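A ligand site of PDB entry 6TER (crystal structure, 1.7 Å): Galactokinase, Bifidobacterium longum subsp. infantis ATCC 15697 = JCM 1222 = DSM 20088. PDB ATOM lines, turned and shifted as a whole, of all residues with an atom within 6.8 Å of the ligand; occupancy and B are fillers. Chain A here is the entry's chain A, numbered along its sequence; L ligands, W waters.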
ATOM      1  N   ARG A  40      -5.676 -10.458  26.709  1.00  0.00           N
ATOM      2  CA  ARG A  40      -4.872 -10.729  27.938  1.00  0.00           C
ATOM      3  C   ARG A  40      -3.367 -10.700  27.642  1.00  0.00           C
ATOM      4  O   ARG A  40      -2.931 -10.989  26.483  1.00  0.00           O
ATOM      5  CB  ARG A  40      -5.246 -12.108  28.499  1.00  0.00           C
ATOM      6  CG  ARG A  40      -4.863 -13.271  27.590  1.00  0.00           C
ATOM      7  CD  ARG A  40      -3.619 -14.060  27.955  1.00  0.00           C
ATOM      8  NE  ARG A  40      -3.250 -15.023  26.912  1.00  0.00           N
ATOM      9  CZ  ARG A  40      -2.493 -14.754  25.842  1.00  0.00           C
ATOM     10  NH1 ARG A  40      -2.236 -15.710  24.981  1.00  0.00           N
ATOM     11  NH2 ARG A  40      -1.992 -13.548  25.593  1.00  0.00           N
ATOM     12  N   ASN A  42      -0.171 -12.844  29.439  1.00  0.00           N
ATOM     13  CA  ASN A  42       0.242 -13.821  30.457  1.00  0.00           C
ATOM     14  C   ASN A  42       1.590 -13.399  31.041  1.00  0.00           C
ATOM     15  O   ASN A  42       2.630 -13.507  30.342  1.00  0.00           O
ATOM     16  CB  ASN A  42       0.359 -15.234  29.914  1.00  0.00           C
ATOM     17  CG  ASN A  42       0.414 -16.218  31.054  1.00  0.00           C
ATOM     18  OD1 ASN A  42      -0.048 -15.922  32.141  1.00  0.00           O
ATOM     19  ND2 ASN A  42       0.987 -17.376  30.812  1.00  0.00           N
ATOM     20  N   GLY A  45       4.349 -18.264  33.200  1.00  0.00           N
ATOM     21  CA  GLY A  45       3.721 -19.589  33.294  1.00  0.00           C
ATOM     22  C   GLY A  45       3.214 -19.961  31.928  1.00  0.00           C
ATOM     23  O   GLY A  45       1.996 -20.146  31.781  1.00  0.00           O
ATOM     24  N   GLU A  46       4.123 -19.992  30.961  1.00  0.00           N
ATOM     25  CA  GLU A  46       3.790 -20.167  29.522  1.00  0.00           C
ATOM     26  C   GLU A  46       3.940 -21.634  29.145  1.00  0.00           C
ATOM     27  O   GLU A  46       4.953 -22.248  29.549  1.00  0.00           O
ATOM     28  CB  GLU A  46       4.713 -19.342  28.654  1.00  0.00           C
ATOM     29  CG  GLU A  46       3.964 -18.718  27.454  1.00  0.00           C
ATOM     30  CD  GLU A  46       2.958 -17.619  27.811  1.00  0.00           C
ATOM     31  OE1 GLU A  46       1.742 -17.860  27.817  1.00  0.00           O
ATOM     32  OE2 GLU A  46       3.398 -16.488  28.060  1.00  0.00           O
ATOM     33  N   HIS A  47       2.993 -22.171  28.348  1.00  0.00           N
ATOM     34  CA  HIS A  47       2.990 -23.613  27.917  1.00  0.00           C
ATOM     35  C   HIS A  47       2.838 -24.532  29.129  1.00  0.00           C
ATOM     36  O   HIS A  47       3.265 -25.748  29.066  1.00  0.00           O
ATOM     37  CB  HIS A  47       4.185 -23.895  26.977  1.00  0.00           C
ATOM     38  CG  HIS A  47       3.944 -23.305  25.634  1.00  0.00           C
ATOM     39  ND1 HIS A  47       3.160 -23.960  24.676  1.00  0.00           N
ATOM     40  CD2 HIS A  47       4.242 -22.090  25.095  1.00  0.00           C
ATOM     41  CE1 HIS A  47       3.063 -23.200  23.588  1.00  0.00           C
ATOM     42  NE2 HIS A  47       3.716 -22.050  23.818  1.00  0.00           N
ATOM     43  N   THR A  48       2.192 -23.996  30.176  1.00  0.00           N
ATOM     44  CA  THR A  48       1.828 -24.673  31.455  1.00  0.00           C
ATOM     45  C   THR A  48       0.329 -25.067  31.506  1.00  0.00           C
ATOM     46  O   THR A  48      -0.008 -26.086  32.180  1.00  0.00           O
ATOM     47  CB  THR A  48       2.280 -23.825  32.677  1.00  0.00           C
ATOM     48  OG1 THR A  48       1.599 -22.567  32.666  1.00  0.00           O
ATOM     49  CG2 THR A  48       3.779 -23.532  32.760  1.00  0.00           C
ATOM     50  N   ASP A  49      -0.575 -24.283  30.916  1.00  0.00           N
ATOM     51  CA  ASP A  49      -2.051 -24.422  31.104  1.00  0.00           C
ATOM     52  C   ASP A  49      -2.546 -25.833  30.695  1.00  0.00           C
ATOM     53  O   ASP A  49      -3.265 -26.455  31.544  1.00  0.00           O
ATOM     54  CB  ASP A  49      -2.790 -23.248  30.451  1.00  0.00           C
ATOM     55  CG  ASP A  49      -2.816 -23.217  28.927  1.00  0.00           C
ATOM     56  OD1 ASP A  49      -1.939 -23.861  28.239  1.00  0.00           O
ATOM     57  OD2 ASP A  49      -3.732 -22.628  28.453  1.00  0.00           O
ATOM     58  N   TYR A  50      -2.098 -26.378  29.544  1.00  0.00           N
ATOM     59  CA  TYR A  50      -2.482 -27.729  29.053  1.00  0.00           C
ATOM     60  C   TYR A  50      -1.636 -28.840  29.737  1.00  0.00           C
ATOM     61  O   TYR A  50      -1.952 -30.069  29.536  1.00  0.00           O
ATOM     62  CB  TYR A  50      -2.438 -27.789  27.518  1.00  0.00           C
ATOM     63  CG  TYR A  50      -1.121 -27.407  26.874  1.00  0.00           C
ATOM     64  CD1 TYR A  50      -0.008 -28.237  26.915  1.00  0.00           C
ATOM     65  CD2 TYR A  50      -0.948 -26.152  26.267  1.00  0.00           C
ATOM     66  CE1 TYR A  50       1.209 -27.865  26.351  1.00  0.00           C
ATOM     67  CE2 TYR A  50       0.263 -25.773  25.706  1.00  0.00           C
ATOM     68  CZ  TYR A  50       1.354 -26.624  25.756  1.00  0.00           C
ATOM     69  OH  TYR A  50       2.529 -26.239  25.187  1.00  0.00           O
ATOM     70  N   CYS A  55      -0.390 -20.456  35.889  1.00  0.00           N
ATOM     71  CA  CYS A  55      -0.397 -19.318  34.931  1.00  0.00           C
ATOM     72  C   CYS A  55      -0.611 -18.080  35.759  1.00  0.00           C
ATOM     73  O   CYS A  55      -1.186 -18.241  36.855  1.00  0.00           O
ATOM     74  CB  CYS A  55      -1.521 -19.415  33.888  1.00  0.00           C
ATOM     75  SG  CYS A  55      -1.501 -21.057  33.135  1.00  0.00           S
ATOM     76  N   GLY A 138      -0.884 -12.377  19.435  1.00  0.00           N
ATOM     77  CA  GLY A 138      -0.876 -13.327  20.573  1.00  0.00           C
ATOM     78  C   GLY A 138      -1.398 -12.748  21.883  1.00  0.00           C
ATOM     79  O   GLY A 138      -0.957 -13.200  22.974  1.00  0.00           O
ATOM     80  N   SER A 140      -4.762 -12.793  22.442  1.00  0.00           N
ATOM     81  CA  SER A 140      -5.989 -13.635  22.558  1.00  0.00           C
ATOM     82  C   SER A 140      -7.240 -12.938  21.980  1.00  0.00           C
ATOM     83  O   SER A 140      -8.293 -12.911  22.660  1.00  0.00           O
ATOM     84  CB  SER A 140      -6.205 -14.081  23.987  1.00  0.00           C
ATOM     85  OG  SER A 140      -5.178 -15.010  24.362  1.00  0.00           O
ATOM     86  N   SER A 142      -8.979 -14.228  19.649  1.00  0.00           N
ATOM     87  CA  SER A 142      -9.743 -15.488  19.790  1.00  0.00           C
ATOM     88  C   SER A 142     -10.693 -15.415  20.994  1.00  0.00           C
ATOM     89  O   SER A 142     -11.902 -15.318  20.817  1.00  0.00           O
ATOM     90  CB  SER A 142      -8.780 -16.639  19.939  1.00  0.00           C
ATOM     91  OG  SER A 142      -7.702 -16.302  20.831  1.00  0.00           O
ATOM     92  N   GLU A 179     -13.453 -23.020  20.180  1.00  0.00           N
ATOM     93  CA  GLU A 179     -12.105 -22.812  19.571  1.00  0.00           C
ATOM     94  C   GLU A 179     -11.460 -24.168  19.166  1.00  0.00           C
ATOM     95  O   GLU A 179     -10.953 -24.274  18.043  1.00  0.00           O
ATOM     96  CB  GLU A 179     -11.245 -22.018  20.552  1.00  0.00           C
ATOM     97  CG  GLU A 179      -9.998 -21.456  19.882  1.00  0.00           C
ATOM     98  CD  GLU A 179      -9.239 -20.348  20.604  1.00  0.00           C
ATOM     99  OE1 GLU A 179      -9.771 -19.811  21.630  1.00  0.00           O
ATOM    100  OE2 GLU A 179      -8.137 -19.973  20.102  1.00  0.00           O
ATOM    101  N   SER A 186      -6.251 -25.712  18.295  1.00  0.00           N
ATOM    102  CA  SER A 186      -5.865 -26.247  19.637  1.00  0.00           C
ATOM    103  C   SER A 186      -5.730 -25.081  20.645  1.00  0.00           C
ATOM    104  O   SER A 186      -5.110 -24.057  20.243  1.00  0.00           O
ATOM    105  CB  SER A 186      -4.578 -27.044  19.530  1.00  0.00           C
ATOM    106  OG  SER A 186      -4.214 -27.603  20.786  1.00  0.00           O
ATOM    107  N   THR A 187      -6.305 -25.167  21.853  1.00  0.00           N
ATOM    108  CA  THR A 187      -6.168 -24.081  22.911  1.00  0.00           C
ATOM    109  C   THR A 187      -6.226 -24.687  24.325  1.00  0.00           C
ATOM    110  O   THR A 187      -7.006 -25.634  24.469  1.00  0.00           O
ATOM    111  CB  THR A 187      -7.247 -22.998  22.754  1.00  0.00           C
ATOM    112  OG1 THR A 187      -7.118 -21.976  23.744  1.00  0.00           O
ATOM    113  CG2 THR A 187      -8.665 -23.537  22.830  1.00  0.00           C
ATOM    114  N   GLY A 188      -5.525 -24.135  25.356  1.00  0.00           N
ATOM    115  CA  GLY A 188      -5.288 -24.836  26.649  1.00  0.00           C
ATOM    116  C   GLY A 188      -6.032 -24.305  27.895  1.00  0.00           C
ATOM    117  O   GLY A 188      -5.915 -25.010  28.959  1.00  0.00           O
ATOM    118  N   GLY A 189      -6.688 -23.150  27.833  1.00  0.00           N
ATOM    119  CA  GLY A 189      -7.632 -22.647  28.857  1.00  0.00           C
ATOM    120  C   GLY A 189      -7.245 -21.321  29.523  1.00  0.00           C
ATOM    121  O   GLY A 189      -8.159 -20.668  30.095  1.00  0.00           O
ATOM    122  N   LEU A 190      -5.965 -20.960  29.485  1.00  0.00           N
ATOM    123  CA  LEU A 190      -5.366 -19.699  30.008  1.00  0.00           C
ATOM    124  C   LEU A 190      -6.202 -18.486  29.574  1.00  0.00           C
ATOM    125  O   LEU A 190      -6.660 -17.739  30.467  1.00  0.00           O
ATOM    126  CB  LEU A 190      -3.918 -19.614  29.486  1.00  0.00           C
ATOM    127  CG  LEU A 190      -2.971 -18.564  30.071  1.00  0.00           C
ATOM    128  CD1 LEU A 190      -1.642 -18.703  29.399  1.00  0.00           C
ATOM    129  CD2 LEU A 190      -3.464 -17.160  29.900  1.00  0.00           C
ATOM    130  N   ASP A 191      -6.442 -18.326  28.268  1.00  0.00           N
ATOM    131  CA  ASP A 191      -6.877 -17.027  27.650  1.00  0.00           C
ATOM    132  C   ASP A 191      -8.298 -16.668  28.121  1.00  0.00           C
ATOM    133  O   ASP A 191      -8.599 -15.481  28.506  1.00  0.00           O
ATOM    134  CB  ASP A 191      -6.809 -17.085  26.120  1.00  0.00           C
ATOM    135  CG  ASP A 191      -5.453 -17.473  25.589  1.00  0.00           C
ATOM    136  OD1 ASP A 191      -4.440 -17.278  26.354  1.00  0.00           O
ATOM    137  OD2 ASP A 191      -5.400 -17.954  24.407  1.00  0.00           O
ATOM    138  N   GLN A 192      -9.161 -17.668  28.103  1.00  0.00           N
ATOM    139  CA  GLN A 192     -10.601 -17.530  28.429  1.00  0.00           C
ATOM    140  C   GLN A 192     -10.818 -17.406  29.938  1.00  0.00           C
ATOM    141  O   GLN A 192     -11.688 -16.614  30.317  1.00  0.00           O
ATOM    142  CB  GLN A 192     -11.345 -18.742  27.869  1.00  0.00           C
ATOM    143  CG  GLN A 192     -11.148 -18.957  26.375  1.00  0.00           C
ATOM    144  CD  GLN A 192      -9.930 -19.808  26.027  1.00  0.00           C
ATOM    145  OE1 GLN A 192      -9.053 -20.073  26.850  1.00  0.00           O
ATOM    146  NE2 GLN A 192      -9.868 -20.259  24.779  1.00  0.00           N
ATOM    147  N   TYR A 248       2.142 -25.312  17.826  1.00  0.00           N
ATOM    148  CA  TYR A 248       1.501 -25.345  19.168  1.00  0.00           C
ATOM    149  C   TYR A 248       1.095 -26.796  19.496  1.00  0.00           C
ATOM    150  O   TYR A 248       1.483 -27.317  20.617  1.00  0.00           O
ATOM    151  CB  TYR A 248       0.367 -24.311  19.175  1.00  0.00           C
ATOM    152  CG  TYR A 248      -0.385 -24.266  20.474  1.00  0.00           C
ATOM    153  CD1 TYR A 248       0.038 -23.444  21.508  1.00  0.00           C
ATOM    154  CD2 TYR A 248      -1.458 -25.091  20.720  1.00  0.00           C
ATOM    155  CE1 TYR A 248      -0.613 -23.440  22.720  1.00  0.00           C
ATOM    156  CE2 TYR A 248      -2.121 -25.094  21.930  1.00  0.00           C
ATOM    157  CZ  TYR A 248      -1.682 -24.281  22.950  1.00  0.00           C
ATOM    158  OH  TYR A 248      -2.393 -24.262  24.106  1.00  0.00           O
ATOM    159  N   ARG A 252       2.086 -29.783  22.513  1.00  0.00           N
ATOM    160  CA  ARG A 252       1.060 -30.384  23.379  1.00  0.00           C
ATOM    161  C   ARG A 252       1.251 -31.909  23.284  1.00  0.00           C
ATOM    162  O   ARG A 252       1.262 -32.568  24.344  1.00  0.00           O
ATOM    163  CB  ARG A 252      -0.372 -29.944  22.997  1.00  0.00           C
ATOM    164  CG  ARG A 252      -0.776 -28.544  23.422  1.00  0.00           C
ATOM    165  CD  ARG A 252      -2.262 -28.196  23.208  1.00  0.00           C
ATOM    166  NE  ARG A 252      -3.071 -28.913  24.205  1.00  0.00           N
ATOM    167  CZ  ARG A 252      -4.394 -28.853  24.339  1.00  0.00           C
ATOM    168  NH1 ARG A 252      -5.125 -28.139  23.491  1.00  0.00           N
ATOM    169  NH2 ARG A 252      -4.981 -29.539  25.306  1.00  0.00           N
ATOM    170  N   LEU A 336      11.782 -20.366  27.077  1.00  0.00           N
ATOM    171  CA  LEU A 336      10.884 -20.568  25.910  1.00  0.00           C
ATOM    172  C   LEU A 336      11.733 -20.701  24.630  1.00  0.00           C
ATOM    173  O   LEU A 336      11.406 -21.532  23.767  1.00  0.00           O
ATOM    174  CB  LEU A 336       9.841 -19.461  25.908  1.00  0.00           C
ATOM    175  CG  LEU A 336       8.724 -19.665  26.944  1.00  0.00           C
ATOM    176  CD1 LEU A 336       8.127 -18.367  27.394  1.00  0.00           C
ATOM    177  CD2 LEU A 336       7.603 -20.549  26.441  1.00  0.00           C
ATOM    178  N   MET A 364       8.695 -12.988  25.654  1.00  0.00           N
ATOM    179  CA  MET A 364       7.514 -13.277  24.782  1.00  0.00           C
ATOM    180  C   MET A 364       6.323 -13.591  25.722  1.00  0.00           C
ATOM    181  O   MET A 364       6.546 -14.191  26.812  1.00  0.00           O
ATOM    182  CB  MET A 364       7.783 -14.429  23.798  1.00  0.00           C
ATOM    183  CG  MET A 364       8.123 -15.737  24.503  1.00  0.00           C
ATOM    184  SD  MET A 364       7.696 -17.199  23.537  1.00  0.00           S
ATOM    185  CE  MET A 364       5.931 -17.163  23.858  1.00  0.00           C
ATOM    186  N   THR A 365       5.107 -13.154  25.388  1.00  0.00           N
ATOM    187  CA  THR A 365       3.883 -13.651  26.070  1.00  0.00           C
ATOM    188  C   THR A 365       3.024 -14.487  25.093  1.00  0.00           C
ATOM    189  O   THR A 365       3.189 -14.329  23.868  1.00  0.00           O
ATOM    190  CB  THR A 365       3.150 -12.511  26.770  1.00  0.00           C
ATOM    191  OG1 THR A 365       2.147 -13.131  27.578  1.00  0.00           O
ATOM    192  CG2 THR A 365       2.572 -11.513  25.790  1.00  0.00           C
ATOM    193  N   GLY A 366       2.258 -15.430  25.645  1.00  0.00           N
ATOM    194  CA  GLY A 366       1.324 -16.365  24.992  1.00  0.00           C
ATOM    195  C   GLY A 366       2.037 -17.456  24.223  1.00  0.00           C
ATOM    196  O   GLY A 366       3.027 -17.921  24.697  1.00  0.00           O
ATOM    197  N   GLY A 367       1.493 -17.866  23.072  1.00  0.00           N
ATOM    198  CA  GLY A 367       1.877 -19.130  22.446  1.00  0.00           C
ATOM    199  C   GLY A 367       3.307 -19.146  21.910  1.00  0.00           C
ATOM    200  O   GLY A 367       3.958 -20.206  21.992  1.00  0.00           O
ATOM    201  N   GLY A 368       3.740 -18.032  21.315  1.00  0.00           N
ATOM    202  CA  GLY A 368       5.031 -17.869  20.614  1.00  0.00           C
ATOM    203  C   GLY A 368       4.849 -17.827  19.107  1.00  0.00           C
ATOM    204  O   GLY A 368       3.707 -17.446  18.605  1.00  0.00           O
HETATM  205  C1  LIG L   1      -1.891 -19.940  23.599  1.00  0.00           C
HETATM  206  C2  LIG L   1      -3.013 -20.820  24.099  1.00  0.00           C
HETATM  207  C3  LIG L   1      -3.076 -20.754  25.624  1.00  0.00           C
HETATM  208  C4  LIG L   1      -1.695 -21.194  26.257  1.00  0.00           C
HETATM  209  C5  LIG L   1      -0.550 -20.445  25.630  1.00  0.00           C
HETATM  210  C6  LIG L   1       0.829 -20.996  26.141  1.00  0.00           C
HETATM  211  O1  LIG L   1      -2.170 -18.530  23.856  1.00  0.00           O
HETATM  212  O2  LIG L   1      -4.314 -20.556  23.471  1.00  0.00           O
HETATM  213  O3  LIG L   1      -4.082 -21.653  26.117  1.00  0.00           O
HETATM  214  O4  LIG L   1      -1.400 -22.595  26.080  1.00  0.00           O
HETATM  215  O5  LIG L   1      -0.647 -20.408  24.196  1.00  0.00           O
HETATM  216  O6  LIG L   1       1.061 -20.531  27.514  1.00  0.00           O
HETATM  217  O   HOH W   1      -1.052 -16.702  21.903  1.00  0.00           O
HETATM  218  O   HOH W   2      -6.407 -20.426  26.217  1.00  0.00           O
HETATM  219  O   HOH W   3       0.326 -21.596  29.907  1.00  0.00           O
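The backbone NH of Gly 189 lies within hydrogen-bond range of an oxygen (O3) of the ligand (3.5 Å).
The side-chain hydroxyl (OG1) of Thr 187 lies within hydrogen-bond range of an oxygen (O2) of the ligand, 3.2 Å away.
O3 of the ligand is in hydrogen-bond range of N of Gly 188 (3.0 Å).
An oxygen (O3) of the ligand lies within hydrogen-bond range of the side-chain carboxylate of Asp 49, 2.6 Å away.
O6 of the ligand lies within hydrogen-bond range of N of His 47 (2.7 Å).
The side-chain hydroxyl of Tyr 248 lies within hydrogen-bond range of an oxygen (O4) of the ligand.
The side-chain carboxylate (OD2) of Asp 191 lies within hydrogen-bond range of an oxygen (O2) of the ligand (3.0 Å).
The side-chain carboxylate (OE1) of Glu 46 is in hydrogen-bond range of an oxygen (O6) of the ligand (2.8 Å).
The guanidinium group (NH1) of Arg 40 sits at hydrogen-bond distance from an oxygen (O1) of the ligand.
OD2 of Asp 49 lies within hydrogen-bond range of N of Gly 189 (3.1 Å).
OH of Tyr 248 sits at hydrogen-bond distance from N of Gly 188, 3.4 Å away.
The side-chain carboxylate (OD1) of Asp 191 is in salt-bridge range of the guanidinium group (NE) of Arg 40.
The side-chain carboxylate of Asp 49 sits at hydrogen-bond distance from the backbone NH of Leu 190 (3.0 Å).
The side-chain amide nitrogen of Asn 42 lies within hydrogen-bond range of the side-chain carboxylate of Glu 46.
The guanidinium group (NH1) of Arg 40 lies close to the side-chain hydroxyl (OG) of Ser 140, at 3.1 Å.
The backbone carbonyl oxygen (O) of Thr 187 lies within hydrogen-bond range of the guanidinium group (NH1) of Arg 252 (3.3 Å).
The guanidinium group (NH2) of Arg 40 lies within hydrogen-bond range of the backbone carbonyl oxygen (O) of Gly 138.
Water W1 lies within hydrogen-bond range of O1 of the ligand (2.9 Å), N of Gly 367 (3.0 Å) and NH1 of Arg 40 (3.4 Å).
Merely in contact with the ligand: Tyr 50, Leu 190, Gly 366 and Gly 367.
Along chain A the residues within 4 Å of the ligand span positions 40 to 367.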
